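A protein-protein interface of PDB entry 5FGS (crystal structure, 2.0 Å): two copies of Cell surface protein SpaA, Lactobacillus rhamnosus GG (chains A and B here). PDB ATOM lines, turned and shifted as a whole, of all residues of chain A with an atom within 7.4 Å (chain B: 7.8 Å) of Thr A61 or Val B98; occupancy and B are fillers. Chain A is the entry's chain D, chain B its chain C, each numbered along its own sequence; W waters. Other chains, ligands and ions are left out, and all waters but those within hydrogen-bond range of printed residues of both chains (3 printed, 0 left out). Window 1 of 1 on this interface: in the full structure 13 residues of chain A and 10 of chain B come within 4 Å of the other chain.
The indole nitrogen (NE1) of Trp A62 sits at hydrogen-bond distance from the side-chain carboxylate (OD1) of Asp B100 (2.7 Å).
The side-chain carboxylate (OE2) of Glu B20 lies within salt-bridge range of the guanidinium group (NH1) of Arg A59, at 3.3 Å.
The backbone NH (N) of Asp B100 is in hydrogen-bond range of the backbone carbonyl oxygen (O) of Leu A60, at 3.0 Å.
N of Trp A62 sits at hydrogen-bond distance from O of Val B98 (2.6 Å).
The backbone NH (N) of Gly B23 sits at hydrogen-bond distance from the backbone carbonyl oxygen (O) of Asn B97 (2.8 Å).
OD1 of Asn A28 sits at hydrogen-bond distance from N of Lys A32.
The backbone carbonyl oxygen (O) of Thr A37 lies within hydrogen-bond range of the backbone NH (N) of Arg A59 (2.8 Å).
O of Thr A61 sits at hydrogen-bond distance from N of Lys A35.
The backbone NH of Phe A33 lies within hydrogen-bond range of the backbone carbonyl oxygen of Val A63, 2.7 Å away.
OD1 of Asn B97 sits at hydrogen-bond distance from OG1 of Thr B96 (2.7 Å).
CE of Lys A32 touches CG2 of Val B98, 3.9 Å away.
Gly B21 touches Arg A59.
O of Leu A60 touches C of Pro B99, 3.95 Å away.
Thr A61 touches Val B98.
O of Thr B96 touches O of Trp A62, at 3.9 Å.
CG1 of Val A63 touches O of Thr B96, 3.5 Å away.
CG1 of Val A63 touches CA of Asn B97 (3.8 Å).
Of chain B, only Val B98 comes within 4 Å of Thr A61.
Of chain A, only Lys A32, Thr A61 and Trp A62 come within 4 Å of Val B98.
Of the printed residues of chain A, Pro B99 touches Leu A60 (3.95 Å).
Printed residues of chain B within 4 Å of Arg A59: Glu B20 (3.3 Å) and Gly B21 (3.3 Å).
Of the printed residues of chain A, Thr B96 touches Trp A62 (3.9 Å) and Val A63 (3.5 Å).
Printed residues of chain B within 4 Å of Val A63: Thr B96 (3.5 Å) and Asn B97 (3.8 Å).
Of the printed residues of chain B, Leu A60 touches Pro B99 and Asp B100.
The nearest residue of chain B that does not touch Thr A61 is Gly B21 (4.1 Å).
The nearest residue of chain A that does not touch Val B98 is Leu A60 (4.2 Å).
The nearest printed residue of chain A that does not touch Thr B96 is Ala A64 (4.4 Å).
Hydrophobic or aromatic side chains of chain B that line the printed part of chain A: Val B98.
Of the 19 printed residues of chain A, 6 touch a printed residue of chain B.
Among the printed residues, Asp or Glu carboxylates within 4 Å of a Lys or Arg side-chain nitrogen of the other chain: Arg A59 with Glu B20 (3.3 Å).
No position is printed for both chains.
Water W3 lies within hydrogen-bond range of the backbone NH (N) of Ala A64 (2.6 Å) and the backbone carbonyl oxygen (O) of Thr B96 (2.7 Å).
Water W2 bridges the side-chain amide oxygen of Asn B97 (2.7 Å) and the side-chain carboxylate of Asp A67 (3.3 Å).
Water W1 bridges OG1 of Thr B72 (2.9 Å) and O of Gly A41 (3.3 Å).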
ATOM      1  N   ILE A  26      20.016  26.982  33.184  1.00  0.00           N
ATOM      2  CA  ILE A  26      20.127  27.183  31.744  1.00  0.00           C
ATOM      3  C   ILE A  26      19.187  26.233  31.026  1.00  0.00           C
ATOM      4  O   ILE A  26      19.264  25.018  31.217  1.00  0.00           O
ATOM      5  CB  ILE A  26      21.573  26.958  31.275  1.00  0.00           C
ATOM      6  CG1 ILE A  26      22.449  28.073  31.859  1.00  0.00           C
ATOM      7  CG2 ILE A  26      21.660  26.954  29.750  1.00  0.00           C
ATOM      8  CD1 ILE A  26      23.928  27.801  31.769  1.00  0.00           C
ATOM      9  N   ASN A  28      17.093  24.893  27.359  1.00  0.00           N
ATOM     10  CA  ASN A  28      17.082  24.821  25.904  1.00  0.00           C
ATOM     11  C   ASN A  28      15.651  24.966  25.389  1.00  0.00           C
ATOM     12  O   ASN A  28      14.716  25.096  26.190  1.00  0.00           O
ATOM     13  CB  ASN A  28      17.750  23.522  25.402  1.00  0.00           C
ATOM     14  CG  ASN A  28      17.032  22.248  25.847  1.00  0.00           C
ATOM     15  OD1 ASN A  28      15.876  22.271  26.275  1.00  0.00           O
ATOM     16  ND2 ASN A  28      17.730  21.120  25.741  1.00  0.00           N
ATOM     17  N   LYS A  32      14.086  21.719  28.593  1.00  0.00           N
ATOM     18  CA  LYS A  32      14.938  20.986  29.524  1.00  0.00           C
ATOM     19  C   LYS A  32      16.066  21.898  29.959  1.00  0.00           C
ATOM     20  O   LYS A  32      16.351  22.904  29.305  1.00  0.00           O
ATOM     21  CB  LYS A  32      15.494  19.713  28.903  1.00  0.00           C
ATOM     22  CG  LYS A  32      14.439  18.670  28.585  1.00  0.00           C
ATOM     23  CD  LYS A  32      15.060  17.277  28.509  1.00  0.00           C
ATOM     24  CE  LYS A  32      14.237  16.315  27.666  1.00  0.00           C
ATOM     25  NZ  LYS A  32      12.841  16.181  28.156  1.00  0.00           N
ATOM     26  N   PHE A  33      16.686  21.526  31.077  1.00  0.00           N
ATOM     27  CA  PHE A  33      17.653  22.355  31.759  1.00  0.00           C
ATOM     28  C   PHE A  33      18.961  21.616  31.968  1.00  0.00           C
ATOM     29  O   PHE A  33      18.996  20.383  32.116  1.00  0.00           O
ATOM     30  CB  PHE A  33      17.091  22.805  33.106  1.00  0.00           C
ATOM     31  CG  PHE A  33      15.961  23.782  32.988  1.00  0.00           C
ATOM     32  CD1 PHE A  33      14.688  23.353  32.652  1.00  0.00           C
ATOM     33  CD2 PHE A  33      16.171  25.136  33.204  1.00  0.00           C
ATOM     34  CE1 PHE A  33      13.643  24.248  32.532  1.00  0.00           C
ATOM     35  CE2 PHE A  33      15.128  26.031  33.090  1.00  0.00           C
ATOM     36  CZ  PHE A  33      13.861  25.589  32.748  1.00  0.00           C
ATOM     37  N   LEU A  34      20.033  22.392  31.992  1.00  0.00           N
ATOM     38  CA  LEU A  34      21.375  21.851  32.007  1.00  0.00           C
ATOM     39  C   LEU A  34      21.731  21.251  33.368  1.00  0.00           C
ATOM     40  O   LEU A  34      21.581  21.914  34.394  1.00  0.00           O
ATOM     41  CB  LEU A  34      22.373  22.954  31.651  1.00  0.00           C
ATOM     42  CG  LEU A  34      23.826  22.522  31.457  1.00  0.00           C
ATOM     43  CD1 LEU A  34      23.931  21.468  30.367  1.00  0.00           C
ATOM     44  CD2 LEU A  34      24.657  23.748  31.101  1.00  0.00           C
ATOM     45  N   LYS A  35      22.210  20.009  33.348  1.00  0.00           N
ATOM     46  CA  LYS A  35      22.743  19.339  34.526  1.00  0.00           C
ATOM     47  C   LYS A  35      24.133  18.824  34.230  1.00  0.00           C
ATOM     48  O   LYS A  35      24.360  18.181  33.213  1.00  0.00           O
ATOM     49  CB  LYS A  35      21.868  18.171  34.950  1.00  0.00           C
ATOM     50  CG  LYS A  35      22.332  17.504  36.245  1.00  0.00           C
ATOM     51  CD  LYS A  35      21.562  16.223  36.529  1.00  0.00           C
ATOM     52  CE  LYS A  35      21.950  15.574  37.843  1.00  0.00           C
ATOM     53  NZ  LYS A  35      21.940  16.544  38.971  1.00  0.00           N
ATOM     54  N   LEU A  36      25.068  19.139  35.114  1.00  0.00           N
ATOM     55  CA  LEU A  36      26.421  18.616  35.021  1.00  0.00           C
ATOM     56  C   LEU A  36      26.485  17.323  35.803  1.00  0.00           C
ATOM     57  O   LEU A  36      25.953  17.240  36.903  1.00  0.00           O
ATOM     58  CB  LEU A  36      27.432  19.614  35.578  1.00  0.00           C
ATOM     59  CG  LEU A  36      27.457  20.972  34.875  1.00  0.00           C
ATOM     60  CD1 LEU A  36      28.595  21.805  35.425  1.00  0.00           C
ATOM     61  CD2 LEU A  36      27.611  20.789  33.370  1.00  0.00           C
ATOM     62  N   THR A  37      27.099  16.309  35.213  1.00  0.00           N
ATOM     63  CA  THR A  37      27.394  15.074  35.926  1.00  0.00           C
ATOM     64  C   THR A  37      28.875  14.786  35.798  1.00  0.00           C
ATOM     65  O   THR A  37      29.561  15.412  34.984  1.00  0.00           O
ATOM     66  CB  THR A  37      26.640  13.869  35.344  1.00  0.00           C
ATOM     67  OG1 THR A  37      27.110  13.614  34.016  1.00  0.00           O
ATOM     68  CG2 THR A  37      25.144  14.116  35.316  1.00  0.00           C
ATOM     69  N   ASP A  38      29.368  13.863  36.621  1.00  0.00           N
ATOM     70  CA  ASP A  38      30.724  13.344  36.451  1.00  0.00           C
ATOM     71  C   ASP A  38      30.712  12.250  35.374  1.00  0.00           C
ATOM     72  O   ASP A  38      29.664  11.988  34.766  1.00  0.00           O
ATOM     73  CB  ASP A  38      31.305  12.844  37.787  1.00  0.00           C
ATOM     74  CG  ASP A  38      30.612  11.594  38.328  1.00  0.00           C
ATOM     75  OD1 ASP A  38      30.028  10.801  37.560  1.00  0.00           O
ATOM     76  OD2 ASP A  38      30.689  11.385  39.553  1.00  0.00           O
ATOM     77  N   GLY A  41      27.998   9.548  35.390  1.00  0.00           N
ATOM     78  CA  GLY A  41      26.617  10.031  35.412  1.00  0.00           C
ATOM     79  C   GLY A  41      26.087  10.463  36.766  1.00  0.00           C
ATOM     80  O   GLY A  41      24.884  10.637  36.926  1.00  0.00           O
ATOM     81  N   ARG A  59      30.196  15.996  32.367  1.00  0.00           N
ATOM     82  CA  ARG A  59      29.340  15.901  31.189  1.00  0.00           C
ATOM     83  C   ARG A  59      28.142  16.829  31.316  1.00  0.00           C
ATOM     84  O   ARG A  59      27.635  17.063  32.414  1.00  0.00           O
ATOM     85  CB  ARG A  59      28.893  14.452  30.962  1.00  0.00           C
ATOM     86  CG  ARG A  59      30.043  13.560  30.535  1.00  0.00           C
ATOM     87  CD  ARG A  59      29.577  12.306  29.811  1.00  0.00           C
ATOM     88  NE  ARG A  59      28.760  11.480  30.696  1.00  0.00           N
ATOM     89  CZ  ARG A  59      29.105  10.293  31.213  1.00  0.00           C
ATOM     90  NH1 ARG A  59      30.277   9.715  30.947  1.00  0.00           N
ATOM     91  NH2 ARG A  59      28.247   9.666  32.014  1.00  0.00           N
ATOM     92  N   LEU A  60      27.696  17.343  30.177  1.00  0.00           N
ATOM     93  CA  LEU A  60      26.503  18.168  30.112  1.00  0.00           C
ATOM     94  C   LEU A  60      25.340  17.273  29.731  1.00  0.00           C
ATOM     95  O   LEU A  60      25.410  16.549  28.744  1.00  0.00           O
ATOM     96  CB  LEU A  60      26.658  19.277  29.066  1.00  0.00           C
ATOM     97  CG  LEU A  60      27.458  20.522  29.435  1.00  0.00           C
ATOM     98  CD1 LEU A  60      28.922  20.190  29.670  1.00  0.00           C
ATOM     99  CD2 LEU A  60      27.321  21.554  28.329  1.00  0.00           C
ATOM    100  N   THR A  61      24.271  17.314  30.526  1.00  0.00           N
ATOM    101  CA  THR A  61      23.042  16.616  30.185  1.00  0.00           C
ATOM    102  C   THR A  61      21.867  17.580  30.302  1.00  0.00           C
ATOM    103  O   THR A  61      21.976  18.636  30.924  1.00  0.00           O
ATOM    104  CB  THR A  61      22.846  15.368  31.057  1.00  0.00           C
ATOM    105  OG1 THR A  61      22.661  15.752  32.423  1.00  0.00           O
ATOM    106  CG2 THR A  61      24.059  14.472  30.951  1.00  0.00           C
ATOM    107  N   TRP A  62      20.765  17.262  29.639  1.00  0.00           N
ATOM    108  CA  TRP A  62      19.599  18.127  29.662  1.00  0.00           C
ATOM    109  C   TRP A  62      18.468  17.392  30.345  1.00  0.00           C
ATOM    110  O   TRP A  62      18.080  16.310  29.912  1.00  0.00           O
ATOM    111  CB  TRP A  62      19.240  18.564  28.248  1.00  0.00           C
ATOM    112  CG  TRP A  62      20.315  19.396  27.648  1.00  0.00           C
ATOM    113  CD1 TRP A  62      21.328  18.972  26.855  1.00  0.00           C
ATOM    114  CD2 TRP A  62      20.505  20.803  27.830  1.00  0.00           C
ATOM    115  NE1 TRP A  62      22.132  20.028  26.510  1.00  0.00           N
ATOM    116  CE2 TRP A  62      21.656  21.166  27.100  1.00  0.00           C
ATOM    117  CE3 TRP A  62      19.809  21.791  28.524  1.00  0.00           C
ATOM    118  CZ2 TRP A  62      22.126  22.478  27.042  1.00  0.00           C
ATOM    119  CZ3 TRP A  62      20.276  23.096  28.475  1.00  0.00           C
ATOM    120  CH2 TRP A  62      21.426  23.429  27.744  1.00  0.00           C
ATOM    121  N   VAL A  63      17.952  17.994  31.416  1.00  0.00           N
ATOM    122  CA  VAL A  63      17.056  17.322  32.353  1.00  0.00           C
ATOM    123  C   VAL A  63      15.874  18.200  32.755  1.00  0.00           C
ATOM    124  O   VAL A  63      15.750  19.335  32.296  1.00  0.00           O
ATOM    125  CB  VAL A  63      17.820  16.915  33.629  1.00  0.00           C
ATOM    126  CG1 VAL A  63      19.056  16.126  33.254  1.00  0.00           C
ATOM    127  CG2 VAL A  63      18.219  18.134  34.459  1.00  0.00           C
ATOM    128  N   ALA A  64      15.002  17.662  33.600  1.00  0.00           N
ATOM    129  CA  ALA A  64      13.860  18.421  34.093  1.00  0.00           C
ATOM    130  C   ALA A  64      14.352  19.547  34.984  1.00  0.00           C
ATOM    131  O   ALA A  64      15.362  19.414  35.686  1.00  0.00           O
ATOM    132  CB  ALA A  64      12.895  17.518  34.847  1.00  0.00           C
ATOM    133  N   ASP A  67      15.784  19.000  38.463  1.00  0.00           N
ATOM    134  CA  ASP A  67      17.045  18.261  38.587  1.00  0.00           C
ATOM    135  C   ASP A  67      18.231  19.042  38.047  1.00  0.00           C
ATOM    136  O   ASP A  67      19.338  18.521  37.992  1.00  0.00           O
ATOM    137  CB  ASP A  67      16.955  16.930  37.830  1.00  0.00           C
ATOM    138  CG  ASP A  67      15.901  16.018  38.384  1.00  0.00           C
ATOM    139  OD1 ASP A  67      15.686  16.038  39.611  1.00  0.00           O
ATOM    140  OD2 ASP A  67      15.301  15.264  37.594  1.00  0.00           O
ATOM    141  N   ALA A  68      18.003  20.293  37.663  1.00  0.00           N
ATOM    142  CA  ALA A  68      19.014  21.064  36.946  1.00  0.00           C
ATOM    143  C   ALA A  68      20.097  21.585  37.862  1.00  0.00           C
ATOM    144  O   ALA A  68      19.875  21.767  39.053  1.00  0.00           O
ATOM    145  CB  ALA A  68      18.362  22.228  36.232  1.00  0.00           C
ATOM    146  N   THR A  69      21.265  21.847  37.282  1.00  0.00           N
ATOM    147  CA  THR A  69      22.372  22.454  38.003  1.00  0.00           C
ATOM    148  C   THR A  69      22.145  23.952  38.115  1.00  0.00           C
ATOM    149  O   THR A  69      21.760  24.604  37.146  1.00  0.00           O
ATOM    150  CB  THR A  69      23.709  22.205  37.290  1.00  0.00           C
ATOM    151  OG1 THR A  69      24.021  20.814  37.338  1.00  0.00           O
ATOM    152  CG2 THR A  69      24.844  22.978  37.939  1.00  0.00           C
ATOM    153  N   LYS B  10      21.973   2.432  24.147  1.00  0.00           N
ATOM    154  CA  LYS B  10      21.707   3.782  23.688  1.00  0.00           C
ATOM    155  C   LYS B  10      22.575   4.110  22.497  1.00  0.00           C
ATOM    156  O   LYS B  10      23.789   3.932  22.566  1.00  0.00           O
ATOM    157  CB  LYS B  10      21.998   4.789  24.809  1.00  0.00           C
ATOM    158  CG  LYS B  10      21.458   6.175  24.528  1.00  0.00           C
ATOM    159  CD  LYS B  10      19.932   6.164  24.534  1.00  0.00           C
ATOM    160  CE  LYS B  10      19.343   7.569  24.520  1.00  0.00           C
ATOM    161  NZ  LYS B  10      19.432   8.268  23.212  1.00  0.00           N
ATOM    162  N   GLU B  20      27.214   7.186  25.587  1.00  0.00           N
ATOM    163  CA  GLU B  20      27.414   7.056  27.011  1.00  0.00           C
ATOM    164  C   GLU B  20      26.745   8.226  27.715  1.00  0.00           C
ATOM    165  O   GLU B  20      26.677   9.324  27.168  1.00  0.00           O
ATOM    166  CB  GLU B  20      28.906   7.047  27.328  1.00  0.00           C
ATOM    167  CG  GLU B  20      29.204   6.877  28.805  1.00  0.00           C
ATOM    168  CD  GLU B  20      30.674   6.896  29.128  1.00  0.00           C
ATOM    169  OE1 GLU B  20      31.487   7.262  28.256  1.00  0.00           O
ATOM    170  OE2 GLU B  20      31.025   6.568  30.282  1.00  0.00           O
ATOM    171  N   GLY B  21      26.248   7.979  28.927  1.00  0.00           N
ATOM    172  CA  GLY B  21      25.801   9.046  29.815  1.00  0.00           C
ATOM    173  C   GLY B  21      24.341   9.440  29.697  1.00  0.00           C
ATOM    174  O   GLY B  21      23.932  10.450  30.268  1.00  0.00           O
ATOM    175  N   ALA B  22      23.559   8.665  28.949  1.00  0.00           N
ATOM    176  CA  ALA B  22      22.132   8.891  28.859  1.00  0.00           C
ATOM    177  C   ALA B  22      21.473   8.190  30.033  1.00  0.00           C
ATOM    178  O   ALA B  22      21.625   6.981  30.204  1.00  0.00           O
ATOM    179  CB  ALA B  22      21.573   8.381  27.540  1.00  0.00           C
ATOM    180  N   GLY B  23      20.717   8.955  30.816  1.00  0.00           N
ATOM    181  CA  GLY B  23      20.116   8.470  32.063  1.00  0.00           C
ATOM    182  C   GLY B  23      18.631   8.224  31.929  1.00  0.00           C
ATOM    183  O   GLY B  23      17.924   8.984  31.264  1.00  0.00           O
ATOM    184  N   PHE B  24      18.178   7.135  32.546  1.00  0.00           N
ATOM    185  CA  PHE B  24      16.820   6.642  32.388  1.00  0.00           C
ATOM    186  C   PHE B  24      16.229   6.238  33.720  1.00  0.00           C
ATOM    187  O   PHE B  24      16.934   5.724  34.588  1.00  0.00           O
ATOM    188  CB  PHE B  24      16.800   5.421  31.491  1.00  0.00           C
ATOM    189  CG  PHE B  24      17.072   5.720  30.052  1.00  0.00           C
ATOM    190  CD1 PHE B  24      18.362   5.917  29.608  1.00  0.00           C
ATOM    191  CD2 PHE B  24      16.034   5.742  29.120  1.00  0.00           C
ATOM    192  CE1 PHE B  24      18.618   6.154  28.266  1.00  0.00           C
ATOM    193  CE2 PHE B  24      16.285   5.988  27.778  1.00  0.00           C
ATOM    194  CZ  PHE B  24      17.577   6.194  27.353  1.00  0.00           C
ATOM    195  N   THR B  72      22.159   4.572  33.722  1.00  0.00           N
ATOM    196  CA  THR B  72      22.876   5.366  32.753  1.00  0.00           C
ATOM    197  C   THR B  72      23.694   4.516  31.783  1.00  0.00           C
ATOM    198  O   THR B  72      24.424   3.614  32.195  1.00  0.00           O
ATOM    199  CB  THR B  72      23.792   6.355  33.477  1.00  0.00           C
ATOM    200  OG1 THR B  72      23.023   7.070  34.453  1.00  0.00           O
ATOM    201  CG2 THR B  72      24.396   7.352  32.490  1.00  0.00           C
ATOM    202  N   GLU B  95      13.746   8.527  29.331  1.00  0.00           N
ATOM    203  CA  GLU B  95      15.022   9.216  29.376  1.00  0.00           C
ATOM    204  C   GLU B  95      14.871  10.490  30.192  1.00  0.00           C
ATOM    205  O   GLU B  95      14.153  11.405  29.808  1.00  0.00           O
ATOM    206  CB  GLU B  95      15.533   9.525  27.969  1.00  0.00           C
ATOM    207  CG  GLU B  95      16.990   9.958  27.955  1.00  0.00           C
ATOM    208  CD  GLU B  95      17.586  10.050  26.565  1.00  0.00           C
ATOM    209  OE1 GLU B  95      16.875   9.748  25.583  1.00  0.00           O
ATOM    210  OE2 GLU B  95      18.774  10.420  26.456  1.00  0.00           O
ATOM    211  N   THR B  96      15.544  10.546  31.327  1.00  0.00           N
ATOM    212  CA  THR B  96      15.456  11.698  32.206  1.00  0.00           C
ATOM    213  C   THR B  96      16.686  12.596  32.144  1.00  0.00           C
ATOM    214  O   THR B  96      16.620  13.757  32.531  1.00  0.00           O
ATOM    215  CB  THR B  96      15.256  11.216  33.640  1.00  0.00           C
ATOM    216  OG1 THR B  96      16.254  10.236  33.940  1.00  0.00           O
ATOM    217  CG2 THR B  96      13.883  10.583  33.782  1.00  0.00           C
ATOM    218  N   ASN B  97      17.804  12.044  31.680  1.00  0.00           N
ATOM    219  CA  ASN B  97      19.068  12.739  31.609  1.00  0.00           C
ATOM    220  C   ASN B  97      19.618  12.590  30.191  1.00  0.00           C
ATOM    221  O   ASN B  97      20.163  11.546  29.837  1.00  0.00           O
ATOM    222  CB  ASN B  97      20.063  12.179  32.646  1.00  0.00           C
ATOM    223  CG  ASN B  97      19.514  12.193  34.082  1.00  0.00           C
ATOM    224  OD1 ASN B  97      18.371  11.822  34.336  1.00  0.00           O
ATOM    225  ND2 ASN B  97      20.355  12.590  35.032  1.00  0.00           N
ATOM    226  N   VAL B  98      19.475  13.637  29.385  1.00  0.00           N
ATOM    227  CA  VAL B  98      19.788  13.564  27.957  1.00  0.00           C
ATOM    228  C   VAL B  98      21.179  14.124  27.669  1.00  0.00           C
ATOM    229  O   VAL B  98      21.485  15.248  28.099  1.00  0.00           O
ATOM    230  CB  VAL B  98      18.752  14.365  27.154  1.00  0.00           C
ATOM    231  CG1 VAL B  98      19.001  14.232  25.657  1.00  0.00           C
ATOM    232  CG2 VAL B  98      17.350  13.912  27.528  1.00  0.00           C
ATOM    233  N   PRO B  99      22.040  13.354  26.959  1.00  0.00           N
ATOM    234  CA  PRO B  99      23.367  13.866  26.635  1.00  0.00           C
ATOM    235  C   PRO B  99      23.290  15.086  25.747  1.00  0.00           C
ATOM    236  O   PRO B  99      22.439  15.149  24.860  1.00  0.00           O
ATOM    237  CB  PRO B  99      24.024  12.715  25.875  1.00  0.00           C
ATOM    238  CG  PRO B  99      23.335  11.501  26.378  1.00  0.00           C
ATOM    239  CD  PRO B  99      21.914  11.929  26.622  1.00  0.00           C
ATOM    240  N   ASP B 100      24.154  16.056  26.028  1.00  0.00           N
ATOM    241  CA  ASP B 100      24.186  17.303  25.295  1.00  0.00           C
ATOM    242  C   ASP B 100      24.453  17.020  23.835  1.00  0.00           C
ATOM    243  O   ASP B 100      25.270  16.185  23.522  1.00  0.00           O
ATOM    244  CB  ASP B 100      25.272  18.226  25.858  1.00  0.00           C
ATOM    245  CG  ASP B 100      25.360  19.537  25.115  1.00  0.00           C
ATOM    246  OD1 ASP B 100      24.311  20.186  24.954  1.00  0.00           O
ATOM    247  OD2 ASP B 100      26.467  19.914  24.681  1.00  0.00           O
ATOM    248  N   GLY B 101      23.753  17.729  22.958  1.00  0.00           N
ATOM    249  CA  GLY B 101      23.821  17.497  21.516  1.00  0.00           C
ATOM    250  C   GLY B 101      22.760  16.533  20.999  1.00  0.00           C
ATOM    251  O   GLY B 101      22.692  16.281  19.791  1.00  0.00           O
ATOM    252  N   TYR B 102      21.925  16.013  21.898  1.00  0.00           N
ATOM    253  CA  TYR B 102      20.892  15.037  21.534  1.00  0.00           C
ATOM    254  C   TYR B 102      19.524  15.437  22.044  1.00  0.00           C
ATOM    255  O   TYR B 102      19.409  16.186  23.001  1.00  0.00           O
ATOM    256  CB  TYR B 102      21.236  13.643  22.077  1.00  0.00           C
ATOM    257  CG  TYR B 102      22.377  13.034  21.325  1.00  0.00           C
ATOM    258  CD1 TYR B 102      22.156  12.305  20.163  1.00  0.00           C
ATOM    259  CD2 TYR B 102      23.685  13.236  21.734  1.00  0.00           C
ATOM    260  CE1 TYR B 102      23.210  11.778  19.438  1.00  0.00           C
ATOM    261  CE2 TYR B 102      24.748  12.711  21.016  1.00  0.00           C
ATOM    262  CZ  TYR B 102      24.501  11.982  19.867  1.00  0.00           C
ATOM    263  OH  TYR B 102      25.548  11.456  19.151  1.00  0.00           O
ATOM    264  N   ASP B 103      18.495  14.933  21.372  1.00  0.00           N
ATOM    265  CA  ASP B 103      17.135  14.995  21.879  1.00  0.00           C
ATOM    266  C   ASP B 103      16.829  13.711  22.608  1.00  0.00           C
ATOM    267  O   ASP B 103      17.408  12.663  22.315  1.00  0.00           O
ATOM    268  CB  ASP B 103      16.125  15.175  20.749  1.00  0.00           C
ATOM    269  CG  ASP B 103      15.705  16.602  20.586  1.00  0.00           C
ATOM    270  OD1 ASP B 103      15.088  17.139  21.524  1.00  0.00           O
ATOM    271  OD2 ASP B 103      15.982  17.178  19.532  1.00  0.00           O
ATOM    272  N   ALA B 104      15.920  13.800  23.565  1.00  0.00           N
ATOM    273  CA  ALA B 104      15.488  12.630  24.297  1.00  0.00           C
ATOM    274  C   ALA B 104      14.887  11.640  23.310  1.00  0.00           C
ATOM    275  O   ALA B 104      14.166  12.032  22.386  1.00  0.00           O
ATOM    276  CB  ALA B 104      14.461  13.017  25.348  1.00  0.00           C
ATOM    277  N   ALA B 105      15.192  10.363  23.505  1.00  0.00           N
ATOM    278  CA  ALA B 105      14.498   9.308  22.792  1.00  0.00           C
ATOM    279  C   ALA B 105      13.042   9.299  23.223  1.00  0.00           C
ATOM    280  O   ALA B 105      12.706   9.776  24.309  1.00  0.00           O
ATOM    281  CB  ALA B 105      15.128   7.963  23.099  1.00  0.00           C
ATOM    282  N   ASP B 121      18.751   8.089  20.220  1.00  0.00           N
ATOM    283  CA  ASP B 121      18.671   9.522  20.493  1.00  0.00           C
ATOM    284  C   ASP B 121      18.966  10.289  19.205  1.00  0.00           C
ATOM    285  O   ASP B 121      20.028  10.110  18.606  1.00  0.00           O
ATOM    286  CB  ASP B 121      19.678   9.908  21.567  1.00  0.00           C
ATOM    287  CG  ASP B 121      19.230   9.493  22.961  1.00  0.00           C
ATOM    288  OD1 ASP B 121      19.595  10.207  23.917  1.00  0.00           O
ATOM    289  N   ALA B 122      18.027  11.127  18.772  1.00  0.00           N
ATOM    290  CA  ALA B 122      18.230  11.949  17.583  1.00  0.00           C
ATOM    291  C   ALA B 122      19.177  13.100  17.899  1.00  0.00           C
ATOM    292  O   ALA B 122      19.037  13.732  18.941  1.00  0.00           O
ATOM    293  CB  ALA B 122      16.904  12.499  17.085  1.00  0.00           C
ATOM    294  N   SER B 124      20.550  16.821  18.011  1.00  0.00           N
ATOM    295  CA  SER B 124      20.098  18.221  18.025  1.00  0.00           C
ATOM    296  C   SER B 124      18.778  18.385  18.771  1.00  0.00           C
ATOM    297  O   SER B 124      18.765  18.437  20.011  1.00  0.00           O
ATOM    298  CB  SER B 124      20.049  18.831  16.612  1.00  0.00           C
ATOM    299  OG  SER B 124      18.776  18.691  16.012  1.00  0.00           O
HETATM  300  O   HOH W   1      22.854   9.973  34.475  1.00  0.00           O
HETATM  301  O   HOH W   2      17.306  12.835  36.598  1.00  0.00           O
HETATM  302  O   HOH W   3      14.741  15.118  33.980  1.00  0.00           O
